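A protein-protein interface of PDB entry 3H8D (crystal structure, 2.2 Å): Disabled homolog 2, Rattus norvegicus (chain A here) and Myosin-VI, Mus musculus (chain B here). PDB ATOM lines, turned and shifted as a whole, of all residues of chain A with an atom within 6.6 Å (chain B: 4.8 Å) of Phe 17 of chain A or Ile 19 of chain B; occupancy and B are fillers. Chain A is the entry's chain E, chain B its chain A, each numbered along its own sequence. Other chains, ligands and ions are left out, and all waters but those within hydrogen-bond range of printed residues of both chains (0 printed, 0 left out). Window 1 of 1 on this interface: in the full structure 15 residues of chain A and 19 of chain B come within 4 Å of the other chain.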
ATOM      1  N   THR A  13      17.878 -12.803   0.084  1.00  0.00           N
ATOM      2  CA  THR A  13      16.599 -12.521   0.740  1.00  0.00           C
ATOM      3  C   THR A  13      16.691 -12.725   2.248  1.00  0.00           C
ATOM      4  O   THR A  13      17.534 -13.484   2.741  1.00  0.00           O
ATOM      5  CB  THR A  13      15.453 -13.384   0.193  1.00  0.00           C
ATOM      6  OG1 THR A  13      15.801 -14.771   0.318  1.00  0.00           O
ATOM      7  CG2 THR A  13      15.160 -13.038  -1.265  1.00  0.00           C
ATOM      8  N   SER A  14      15.804 -12.040   2.965  1.00  0.00           N
ATOM      9  CA  SER A  14      15.721 -12.123   4.415  1.00  0.00           C
ATOM     10  C   SER A  14      15.398 -13.537   4.896  1.00  0.00           C
ATOM     11  O   SER A  14      14.954 -14.393   4.119  1.00  0.00           O
ATOM     12  CB  SER A  14      14.664 -11.149   4.934  1.00  0.00           C
ATOM     13  OG  SER A  14      13.369 -11.598   4.586  1.00  0.00           O
ATOM     14  N   SER A  15      15.627 -13.767   6.186  1.00  0.00           N
ATOM     15  CA  SER A  15      15.344 -15.046   6.824  1.00  0.00           C
ATOM     16  C   SER A  15      13.837 -15.315   6.865  1.00  0.00           C
ATOM     17  O   SER A  15      13.405 -16.459   6.724  1.00  0.00           O
ATOM     18  CB  SER A  15      15.947 -15.076   8.234  1.00  0.00           C
ATOM     19  OG  SER A  15      15.999 -16.400   8.737  1.00  0.00           O
ATOM     20  N   ALA A  16      13.050 -14.257   7.057  1.00  0.00           N
ATOM     21  CA  ALA A  16      11.584 -14.336   7.019  1.00  0.00           C
ATOM     22  C   ALA A  16      11.058 -14.788   5.647  1.00  0.00           C
ATOM     23  O   ALA A  16      10.094 -15.558   5.570  1.00  0.00           O
ATOM     24  CB  ALA A  16      10.962 -12.990   7.417  1.00  0.00           C
ATOM     25  N   PHE A  17      11.697 -14.311   4.577  1.00  0.00           N
ATOM     26  CA  PHE A  17      11.347 -14.726   3.214  1.00  0.00           C
ATOM     27  C   PHE A  17      11.797 -16.156   2.901  1.00  0.00           C
ATOM     28  O   PHE A  17      11.013 -16.947   2.372  1.00  0.00           O
ATOM     29  CB  PHE A  17      11.887 -13.749   2.157  1.00  0.00           C
ATOM     30  CG  PHE A  17      11.367 -14.025   0.770  1.00  0.00           C
ATOM     31  CD1 PHE A  17      10.162 -13.474   0.343  1.00  0.00           C
ATOM     32  CD2 PHE A  17      12.061 -14.869  -0.095  1.00  0.00           C
ATOM     33  CE1 PHE A  17       9.666 -13.745  -0.938  1.00  0.00           C
ATOM     34  CE2 PHE A  17      11.573 -15.143  -1.374  1.00  0.00           C
ATOM     35  CZ  PHE A  17      10.376 -14.578  -1.793  1.00  0.00           C
ATOM     36  N   SER A  18      13.052 -16.475   3.220  1.00  0.00           N
ATOM     37  CA  SER A  18      13.586 -17.835   3.064  1.00  0.00           C
ATOM     38  C   SER A  18      12.719 -18.871   3.760  1.00  0.00           C
ATOM     39  O   SER A  18      12.509 -19.964   3.234  1.00  0.00           O
ATOM     40  CB  SER A  18      15.011 -17.936   3.606  1.00  0.00           C
ATOM     41  OG  SER A  18      15.923 -17.201   2.815  1.00  0.00           O
ATOM     42  N   SER A  19      12.215 -18.522   4.942  1.00  0.00           N
ATOM     43  CA  SER A  19      11.324 -19.405   5.692  1.00  0.00           C
ATOM     44  C   SER A  19       9.987 -19.553   4.972  1.00  0.00           C
ATOM     45  O   SER A  19       9.512 -20.675   4.748  1.00  0.00           O
ATOM     46  CB  SER A  19      11.119 -18.880   7.117  1.00  0.00           C
ATOM     47  OG  SER A  19      10.162 -19.669   7.805  1.00  0.00           O
ATOM     48  N   TYR A  20       9.389 -18.417   4.606  1.00  0.00           N
ATOM     49  CA  TYR A  20       8.157 -18.405   3.817  1.00  0.00           C
ATOM     50  C   TYR A  20       8.287 -19.259   2.546  1.00  0.00           C
ATOM     51  O   TYR A  20       7.472 -20.155   2.320  1.00  0.00           O
ATOM     52  CB  TYR A  20       7.713 -16.963   3.471  1.00  0.00           C
ATOM     53  CG  TYR A  20       6.895 -16.896   2.198  1.00  0.00           C
ATOM     54  CD1 TYR A  20       5.554 -17.282   2.186  1.00  0.00           C
ATOM     55  CD2 TYR A  20       7.478 -16.493   0.988  1.00  0.00           C
ATOM     56  CE1 TYR A  20       4.809 -17.255   1.007  1.00  0.00           C
ATOM     57  CE2 TYR A  20       6.739 -16.465  -0.196  1.00  0.00           C
ATOM     58  CZ  TYR A  20       5.410 -16.847  -0.178  1.00  0.00           C
ATOM     59  OH  TYR A  20       4.673 -16.826  -1.344  1.00  0.00           O
ATOM     60  N   PHE A  21       9.316 -18.981   1.734  1.00  0.00           N
ATOM     61  CA  PHE A  21       9.457 -19.603   0.416  1.00  0.00           C
ATOM     62  C   PHE A  21       9.608 -21.126   0.496  1.00  0.00           C
ATOM     63  O   PHE A  21       8.958 -21.853  -0.259  1.00  0.00           O
ATOM     64  CB  PHE A  21      10.611 -18.973  -0.383  1.00  0.00           C
ATOM     65  CG  PHE A  21      10.537 -19.240  -1.873  1.00  0.00           C
ATOM     66  CD1 PHE A  21       9.857 -18.367  -2.717  1.00  0.00           C
ATOM     67  CD2 PHE A  21      11.140 -20.370  -2.426  1.00  0.00           C
ATOM     68  CE1 PHE A  21       9.784 -18.607  -4.086  1.00  0.00           C
ATOM     69  CE2 PHE A  21      11.070 -20.628  -3.796  1.00  0.00           C
ATOM     70  CZ  PHE A  21      10.386 -19.742  -4.631  1.00  0.00           C
ATOM     71  N   ASN A  22      10.454 -21.602   1.408  1.00  0.00           N
ATOM     72  CA  ASN A  22      10.627 -23.045   1.609  1.00  0.00           C
ATOM     73  C   ASN A  22       9.372 -23.757   2.129  1.00  0.00           C
ATOM     74  O   ASN A  22       9.052 -24.856   1.681  1.00  0.00           O
ATOM     75  CB  ASN A  22      11.850 -23.335   2.481  1.00  0.00           C
ATOM     76  CG  ASN A  22      13.160 -23.093   1.741  1.00  0.00           C
ATOM     77  OD1 ASN A  22      13.758 -24.023   1.192  1.00  0.00           O
ATOM     78  ND2 ASN A  22      13.598 -21.838   1.700  1.00  0.00           N
ATOM     79  N   VAL A  25       6.423 -22.734  -1.067  1.00  0.00           N
ATOM     80  CA  VAL A  25       6.668 -22.812  -2.515  1.00  0.00           C
ATOM     81  C   VAL A  25       7.649 -23.944  -2.894  1.00  0.00           C
ATOM     82  O   VAL A  25       7.282 -24.910  -3.570  1.00  0.00           O
ATOM     83  CB  VAL A  25       7.146 -21.423  -3.108  1.00  0.00           C
ATOM     84  CG1 VAL A  25       7.117 -21.447  -4.622  1.00  0.00           C
ATOM     85  CG2 VAL A  25       6.284 -20.256  -2.585  1.00  0.00           C
ATOM     86  N   ILE A  27      12.248 -25.096  -3.067  1.00  0.00           N
ATOM     87  CA  ILE A  27      13.660 -24.811  -2.842  1.00  0.00           C
ATOM     88  C   ILE A  27      14.103 -23.862  -3.936  1.00  0.00           C
ATOM     89  O   ILE A  27      14.108 -24.233  -5.107  1.00  0.00           O
ATOM     90  CB  ILE A  27      14.538 -26.101  -2.845  1.00  0.00           C
ATOM     91  CG1 ILE A  27      13.892 -27.221  -2.014  1.00  0.00           C
ATOM     92  CG2 ILE A  27      15.993 -25.781  -2.432  1.00  0.00           C
ATOM     93  CD1 ILE A  27      13.504 -26.849  -0.578  1.00  0.00           C
ATOM     94  N   PRO A  28      14.441 -22.622  -3.555  1.00  0.00           N
ATOM     95  CA  PRO A  28      14.842 -21.578  -4.494  1.00  0.00           C
ATOM     96  C   PRO A  28      16.118 -21.923  -5.263  1.00  0.00           C
ATOM     97  O   PRO A  28      17.054 -22.494  -4.689  1.00  0.00           O
ATOM     98  CB  PRO A  28      15.080 -20.374  -3.589  1.00  0.00           C
ATOM     99  CG  PRO A  28      15.316 -20.959  -2.217  1.00  0.00           C
ATOM    100  CD  PRO A  28      14.430 -22.138  -2.162  1.00  0.00           C
ATOM    101  N   GLN A  29      16.131 -21.593  -6.554  1.00  0.00           N
ATOM    102  CA  GLN A  29      17.277 -21.829  -7.427  1.00  0.00           C
ATOM    103  C   GLN A  29      17.774 -20.486  -7.963  1.00  0.00           C
ATOM    104  O   GLN A  29      17.050 -19.481  -7.922  1.00  0.00           O
ATOM    105  CB  GLN A  29      16.926 -22.784  -8.581  1.00  0.00           C
ATOM    106  CG  GLN A  29      16.352 -24.149  -8.157  1.00  0.00           C
ATOM    107  CD  GLN A  29      17.371 -25.026  -7.430  1.00  0.00           C
ATOM    108  OE1 GLN A  29      17.460 -25.011  -6.205  1.00  0.00           O
ATOM    109  NE2 GLN A  29      18.155 -25.769  -8.188  1.00  0.00           N
ATOM    110  N   PHE B  17       9.461  -9.447  -9.486  1.00  0.00           N
ATOM    111  CA  PHE B  17      10.488 -10.388  -9.058  1.00  0.00           C
ATOM    112  C   PHE B  17      10.154 -11.813  -9.487  1.00  0.00           C
ATOM    113  O   PHE B  17       8.978 -12.172  -9.626  1.00  0.00           O
ATOM    114  CB  PHE B  17      10.733 -10.272  -7.536  1.00  0.00           C
ATOM    115  CG  PHE B  17      11.216  -8.911  -7.118  1.00  0.00           C
ATOM    116  CD1 PHE B  17      10.306  -7.881  -6.855  1.00  0.00           C
ATOM    117  CD2 PHE B  17      12.579  -8.642  -7.027  1.00  0.00           C
ATOM    118  CE1 PHE B  17      10.747  -6.612  -6.505  1.00  0.00           C
ATOM    119  CE2 PHE B  17      13.031  -7.368  -6.667  1.00  0.00           C
ATOM    120  CZ  PHE B  17      12.109  -6.354  -6.410  1.00  0.00           C
ATOM    121  N   ARG B  18      11.199 -12.604  -9.724  1.00  0.00           N
ATOM    122  CA  ARG B  18      11.062 -14.001 -10.110  1.00  0.00           C
ATOM    123  C   ARG B  18      12.074 -14.872  -9.335  1.00  0.00           C
ATOM    124  O   ARG B  18      13.262 -14.533  -9.219  1.00  0.00           O
ATOM    125  CB  ARG B  18      11.252 -14.150 -11.622  1.00  0.00           C
ATOM    126  CG  ARG B  18      11.230 -15.592 -12.136  1.00  0.00           C
ATOM    127  CD  ARG B  18      11.763 -15.735 -13.556  1.00  0.00           C
ATOM    128  NE  ARG B  18      13.029 -15.031 -13.788  1.00  0.00           N
ATOM    129  CZ  ARG B  18      13.439 -14.643 -14.994  1.00  0.00           C
ATOM    130  NH1 ARG B  18      12.697 -14.906 -16.065  1.00  0.00           N
ATOM    131  NH2 ARG B  18      14.572 -13.967 -15.134  1.00  0.00           N
ATOM    132  N   ILE B  19      11.593 -15.984  -8.793  1.00  0.00           N
ATOM    133  CA  ILE B  19      12.466 -16.956  -8.132  1.00  0.00           C
ATOM    134  C   ILE B  19      12.225 -18.345  -8.705  1.00  0.00           C
ATOM    135  O   ILE B  19      11.160 -18.923  -8.497  1.00  0.00           O
ATOM    136  CB  ILE B  19      12.288 -16.952  -6.595  1.00  0.00           C
ATOM    137  CG1 ILE B  19      12.629 -15.561  -6.030  1.00  0.00           C
ATOM    138  CG2 ILE B  19      13.185 -18.026  -5.932  1.00  0.00           C
ATOM    139  CD1 ILE B  19      12.125 -15.348  -4.678  1.00  0.00           C
ATOM    140  N   PRO B  20      13.217 -18.883  -9.440  1.00  0.00           N
ATOM    141  CA  PRO B  20      13.087 -20.269  -9.855  1.00  0.00           C
ATOM    142  C   PRO B  20      13.193 -21.185  -8.625  1.00  0.00           C
ATOM    143  O   PRO B  20      13.867 -20.842  -7.648  1.00  0.00           O
ATOM    144  CB  PRO B  20      14.264 -20.479 -10.815  1.00  0.00           C
ATOM    145  CG  PRO B  20      14.914 -19.146 -11.003  1.00  0.00           C
ATOM    146  CD  PRO B  20      14.479 -18.267  -9.891  1.00  0.00           C
ATOM    147  N   PHE B  21      12.477 -22.304  -8.657  1.00  0.00           N
ATOM    148  CA  PHE B  21      12.478 -23.237  -7.548  1.00  0.00           C
ATOM    149  C   PHE B  21      12.337 -24.668  -8.055  1.00  0.00           C
ATOM    150  O   PHE B  21      11.919 -24.906  -9.196  1.00  0.00           O
ATOM    151  CB  PHE B  21      11.367 -22.918  -6.514  1.00  0.00           C
ATOM    152  CG  PHE B  21       9.960 -23.162  -7.025  1.00  0.00           C
ATOM    153  CD1 PHE B  21       9.239 -22.134  -7.643  1.00  0.00           C
ATOM    154  CD2 PHE B  21       9.361 -24.415  -6.899  1.00  0.00           C
ATOM    155  CE1 PHE B  21       7.941 -22.355  -8.118  1.00  0.00           C
ATOM    156  CE2 PHE B  21       8.066 -24.641  -7.369  1.00  0.00           C
ATOM    157  CZ  PHE B  21       7.357 -23.608  -7.986  1.00  0.00           C
ATOM    158  N   GLY B  37      10.145 -25.053 -11.342  1.00  0.00           N
ATOM    159  CA  GLY B  37       9.021 -24.144 -11.468  1.00  0.00           C
ATOM    160  C   GLY B  37       9.514 -22.731 -11.205  1.00  0.00           C
ATOM    161  O   GLY B  37      10.693 -22.535 -10.903  1.00  0.00           O
ATOM    162  N   TRP B  38       8.617 -21.750 -11.343  1.00  0.00           N
ATOM    163  CA  TRP B  38       8.946 -20.336 -11.145  1.00  0.00           C
ATOM    164  C   TRP B  38       7.877 -19.597 -10.337  1.00  0.00           C
ATOM    165  O   TRP B  38       6.677 -19.700 -10.609  1.00  0.00           O
ATOM    166  CB  TRP B  38       9.190 -19.636 -12.497  1.00  0.00           C
ATOM    167  CG  TRP B  38      10.360 -20.219 -13.248  1.00  0.00           C
ATOM    168  CD1 TRP B  38      11.651 -19.760 -13.247  1.00  0.00           C
ATOM    169  CD2 TRP B  38      10.347 -21.386 -14.085  1.00  0.00           C
ATOM    170  NE1 TRP B  38      12.438 -20.564 -14.044  1.00  0.00           N
ATOM    171  CE2 TRP B  38      11.666 -21.573 -14.561  1.00  0.00           C
ATOM    172  CE3 TRP B  38       9.351 -22.295 -14.474  1.00  0.00           C
ATOM    173  CZ2 TRP B  38      12.015 -22.632 -15.399  1.00  0.00           C
ATOM    174  CZ3 TRP B  38       9.698 -23.346 -15.314  1.00  0.00           C
ATOM    175  CH2 TRP B  38      11.020 -23.509 -15.762  1.00  0.00           C
ATOM    176  N   TRP B  39       8.338 -18.841  -9.351  1.00  0.00           N
ATOM    177  CA  TRP B  39       7.489 -17.995  -8.509  1.00  0.00           C
ATOM    178  C   TRP B  39       7.658 -16.556  -8.967  1.00  0.00           C
ATOM    179  O   TRP B  39       8.780 -16.124  -9.238  1.00  0.00           O
ATOM    180  CB  TRP B  39       7.960 -18.152  -7.068  1.00  0.00           C
ATOM    181  CG  TRP B  39       7.319 -17.295  -6.000  1.00  0.00           C
ATOM    182  CD1 TRP B  39       6.294 -17.657  -5.174  1.00  0.00           C
ATOM    183  CD2 TRP B  39       7.726 -15.986  -5.579  1.00  0.00           C
ATOM    184  NE1 TRP B  39       6.025 -16.658  -4.281  1.00  0.00           N
ATOM    185  CE2 TRP B  39       6.881 -15.613  -4.509  1.00  0.00           C
ATOM    186  CE3 TRP B  39       8.712 -15.085  -6.011  1.00  0.00           C
ATOM    187  CZ2 TRP B  39       6.982 -14.372  -3.863  1.00  0.00           C
ATOM    188  CZ3 TRP B  39       8.821 -13.860  -5.368  1.00  0.00           C
ATOM    189  CH2 TRP B  39       7.956 -13.515  -4.297  1.00  0.00           C
ATOM    190  N   CYS B  73       2.370 -14.256  -0.169  1.00  0.00           N
ATOM    191  CA  CYS B  73       3.417 -13.710   0.680  1.00  0.00           C
ATOM    192  C   CYS B  73       2.873 -12.508   1.450  1.00  0.00           C
ATOM    193  O   CYS B  73       2.246 -11.614   0.870  1.00  0.00           O
ATOM    194  CB  CYS B  73       4.648 -13.301  -0.129  1.00  0.00           C
ATOM    195  SG  CYS B  73       6.024 -12.765   0.925  1.00  0.00           S
ATOM    196  N   LEU B  75       4.824 -10.552   3.606  1.00  0.00           N
ATOM    197  CA  LEU B  75       5.869  -9.566   3.872  1.00  0.00           C
ATOM    198  C   LEU B  75       5.874  -8.426   2.851  1.00  0.00           C
ATOM    199  O   LEU B  75       5.608  -8.641   1.665  1.00  0.00           O
ATOM    200  CB  LEU B  75       7.241 -10.252   3.865  1.00  0.00           C
ATOM    201  CG  LEU B  75       7.465 -11.509   4.708  1.00  0.00           C
ATOM    202  CD1 LEU B  75       8.738 -12.203   4.263  1.00  0.00           C
ATOM    203  CD2 LEU B  75       7.503 -11.196   6.201  1.00  0.00           C
ATOM    204  N   THR B  80      11.139  -8.566   2.540  1.00  0.00           N
ATOM    205  CA  THR B  80      11.405  -9.777   1.746  1.00  0.00           C
ATOM    206  C   THR B  80      12.900  -9.886   1.451  1.00  0.00           C
ATOM    207  O   THR B  80      13.446 -10.972   1.401  1.00  0.00           O
ATOM    208  CB  THR B  80      10.669  -9.791   0.383  1.00  0.00           C
ATOM    209  OG1 THR B  80      11.137  -8.703  -0.428  1.00  0.00           O
ATOM    210  CG2 THR B  80       9.156  -9.705   0.544  1.00  0.00           C
ATOM    211  N   LEU B  82      14.071  -9.009  -1.413  1.00  0.00           N
ATOM    212  CA  LEU B  82      14.150  -9.310  -2.852  1.00  0.00           C
ATOM    213  C   LEU B  82      14.965  -8.286  -3.662  1.00  0.00           C
ATOM    214  O   LEU B  82      15.620  -8.651  -4.649  1.00  0.00           O
ATOM    215  CB  LEU B  82      12.749  -9.476  -3.454  1.00  0.00           C
ATOM    216  CG  LEU B  82      11.981 -10.770  -3.164  1.00  0.00           C
ATOM    217  CD1 LEU B  82      10.500 -10.557  -3.374  1.00  0.00           C
ATOM    218  CD2 LEU B  82      12.474 -11.922  -4.027  1.00  0.00           C
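The backbone carbonyl oxygen of Thr 80 of chain B sits at hydrogen-bond distance from the backbone NH of Ser 14 of chain A (3.0 Å). The indole nitrogen (NE1) of Trp 39 of chain B is in hydrogen-bond range of the side-chain hydroxyl (OH) of Tyr 20 of chain A. The backbone NH (N) of Gln 29 of chain A lies within hydrogen-bond range of the backbone carbonyl oxygen (O) of Pro 20 of chain B (2.6 Å).
O of Trp 39 of chain B lies within hydrogen-bond range of N of Ile 19 of chain B (2.9 Å). The side-chain sulfur of Cys 73 of chain B lies close to the backbone NH of Leu 75 of chain B, at 3.7 Å. The side-chain hydroxyl (OG) of Ser 18 of chain A lies within hydrogen-bond range of the backbone carbonyl oxygen (O) of Ser 14 of chain A (3.2 Å). The backbone NH (N) of Phe 17 of chain A lies within hydrogen-bond range of the side-chain hydroxyl (OG) of Ser 14 of chain A (3.2 Å). O of Phe 21 of chain B sits at hydrogen-bond distance from N of Gly 37 of chain B, 2.8 Å away. The side-chain hydroxyl (OG1) of Thr 80 of chain B lies within hydrogen-bond range of the backbone NH (N) of Leu 82 of chain B (3.1 Å).
Among the printed residues, merely in contact across the chains: Ile 27 of chain A with Phe 21 of chain B (3.1 Å), Phe 17 of chain A with Thr 80 of chain B (3.3 Å), Phe 17 of chain A with Ile 19 of chain B (3.4 Å), Thr 13 of chain A with Thr 80 of chain B (3.4 Å), Pro 28 of chain A with Pro 20 of chain B (3.4 Å), Phe 21 of chain A with Trp 39 of chain B (3.4 Å), Phe 21 of chain A with Ile 19 of chain B (3.5 Å), Phe 21 of chain A with Phe 21 of chain B (3.6 Å), Tyr 20 of chain A with Cys 73 of chain B (3.6 Å), Phe 17 of chain A with Trp 39 of chain B (3.6 Å), Phe 17 of chain A with Leu 75 of chain B (3.6 Å), Val 25 of chain A with Trp 39 of chain B (3.7 Å), Val 25 of chain A with Phe 21 of chain B (3.7 Å), Ala 16 of chain A with Leu 75 of chain B (3.7 Å) and Pro 28 of chain A with Ile 19 of chain B (3.8 Å).
Printed residues of chain B within 4 Å of Ser 14 of chain A: Thr 80 (3.0 Å). Arg 18 of chain B touches none of the printed residues of chain A. Ile 19 of chain B touches three residues of chain A. Of the printed residues of chain A, Phe 21 of chain B touches Phe 21, Val 25 and Ile 27. Trp 38 of chain B touches none of the printed residues of chain A. The nearest residue of chain B that does not touch Phe 17 of chain A is Leu 82 of chain B (4.1 Å). The nearest residue of chain A that does not touch Ile 19 of chain B is Gln 29 of chain A (4.6 Å). The nearest printed residue of chain A that does not touch Cys 73 of chain B is Phe 17 of chain A (4.2 Å).
Hydrophobic or aromatic side chains of chain A within 4 Å of the printed part of chain B: Ala 16, Phe 17, Tyr 20, Phe 21, Val 25 and Pro 28. Of the 12 printed residues of chain B, 7 touch a printed residue of chain A. Among the printed residues, no Asp or Glu carboxylate lies within 4 Å of a Lys or Arg side-chain nitrogen of the other chain.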
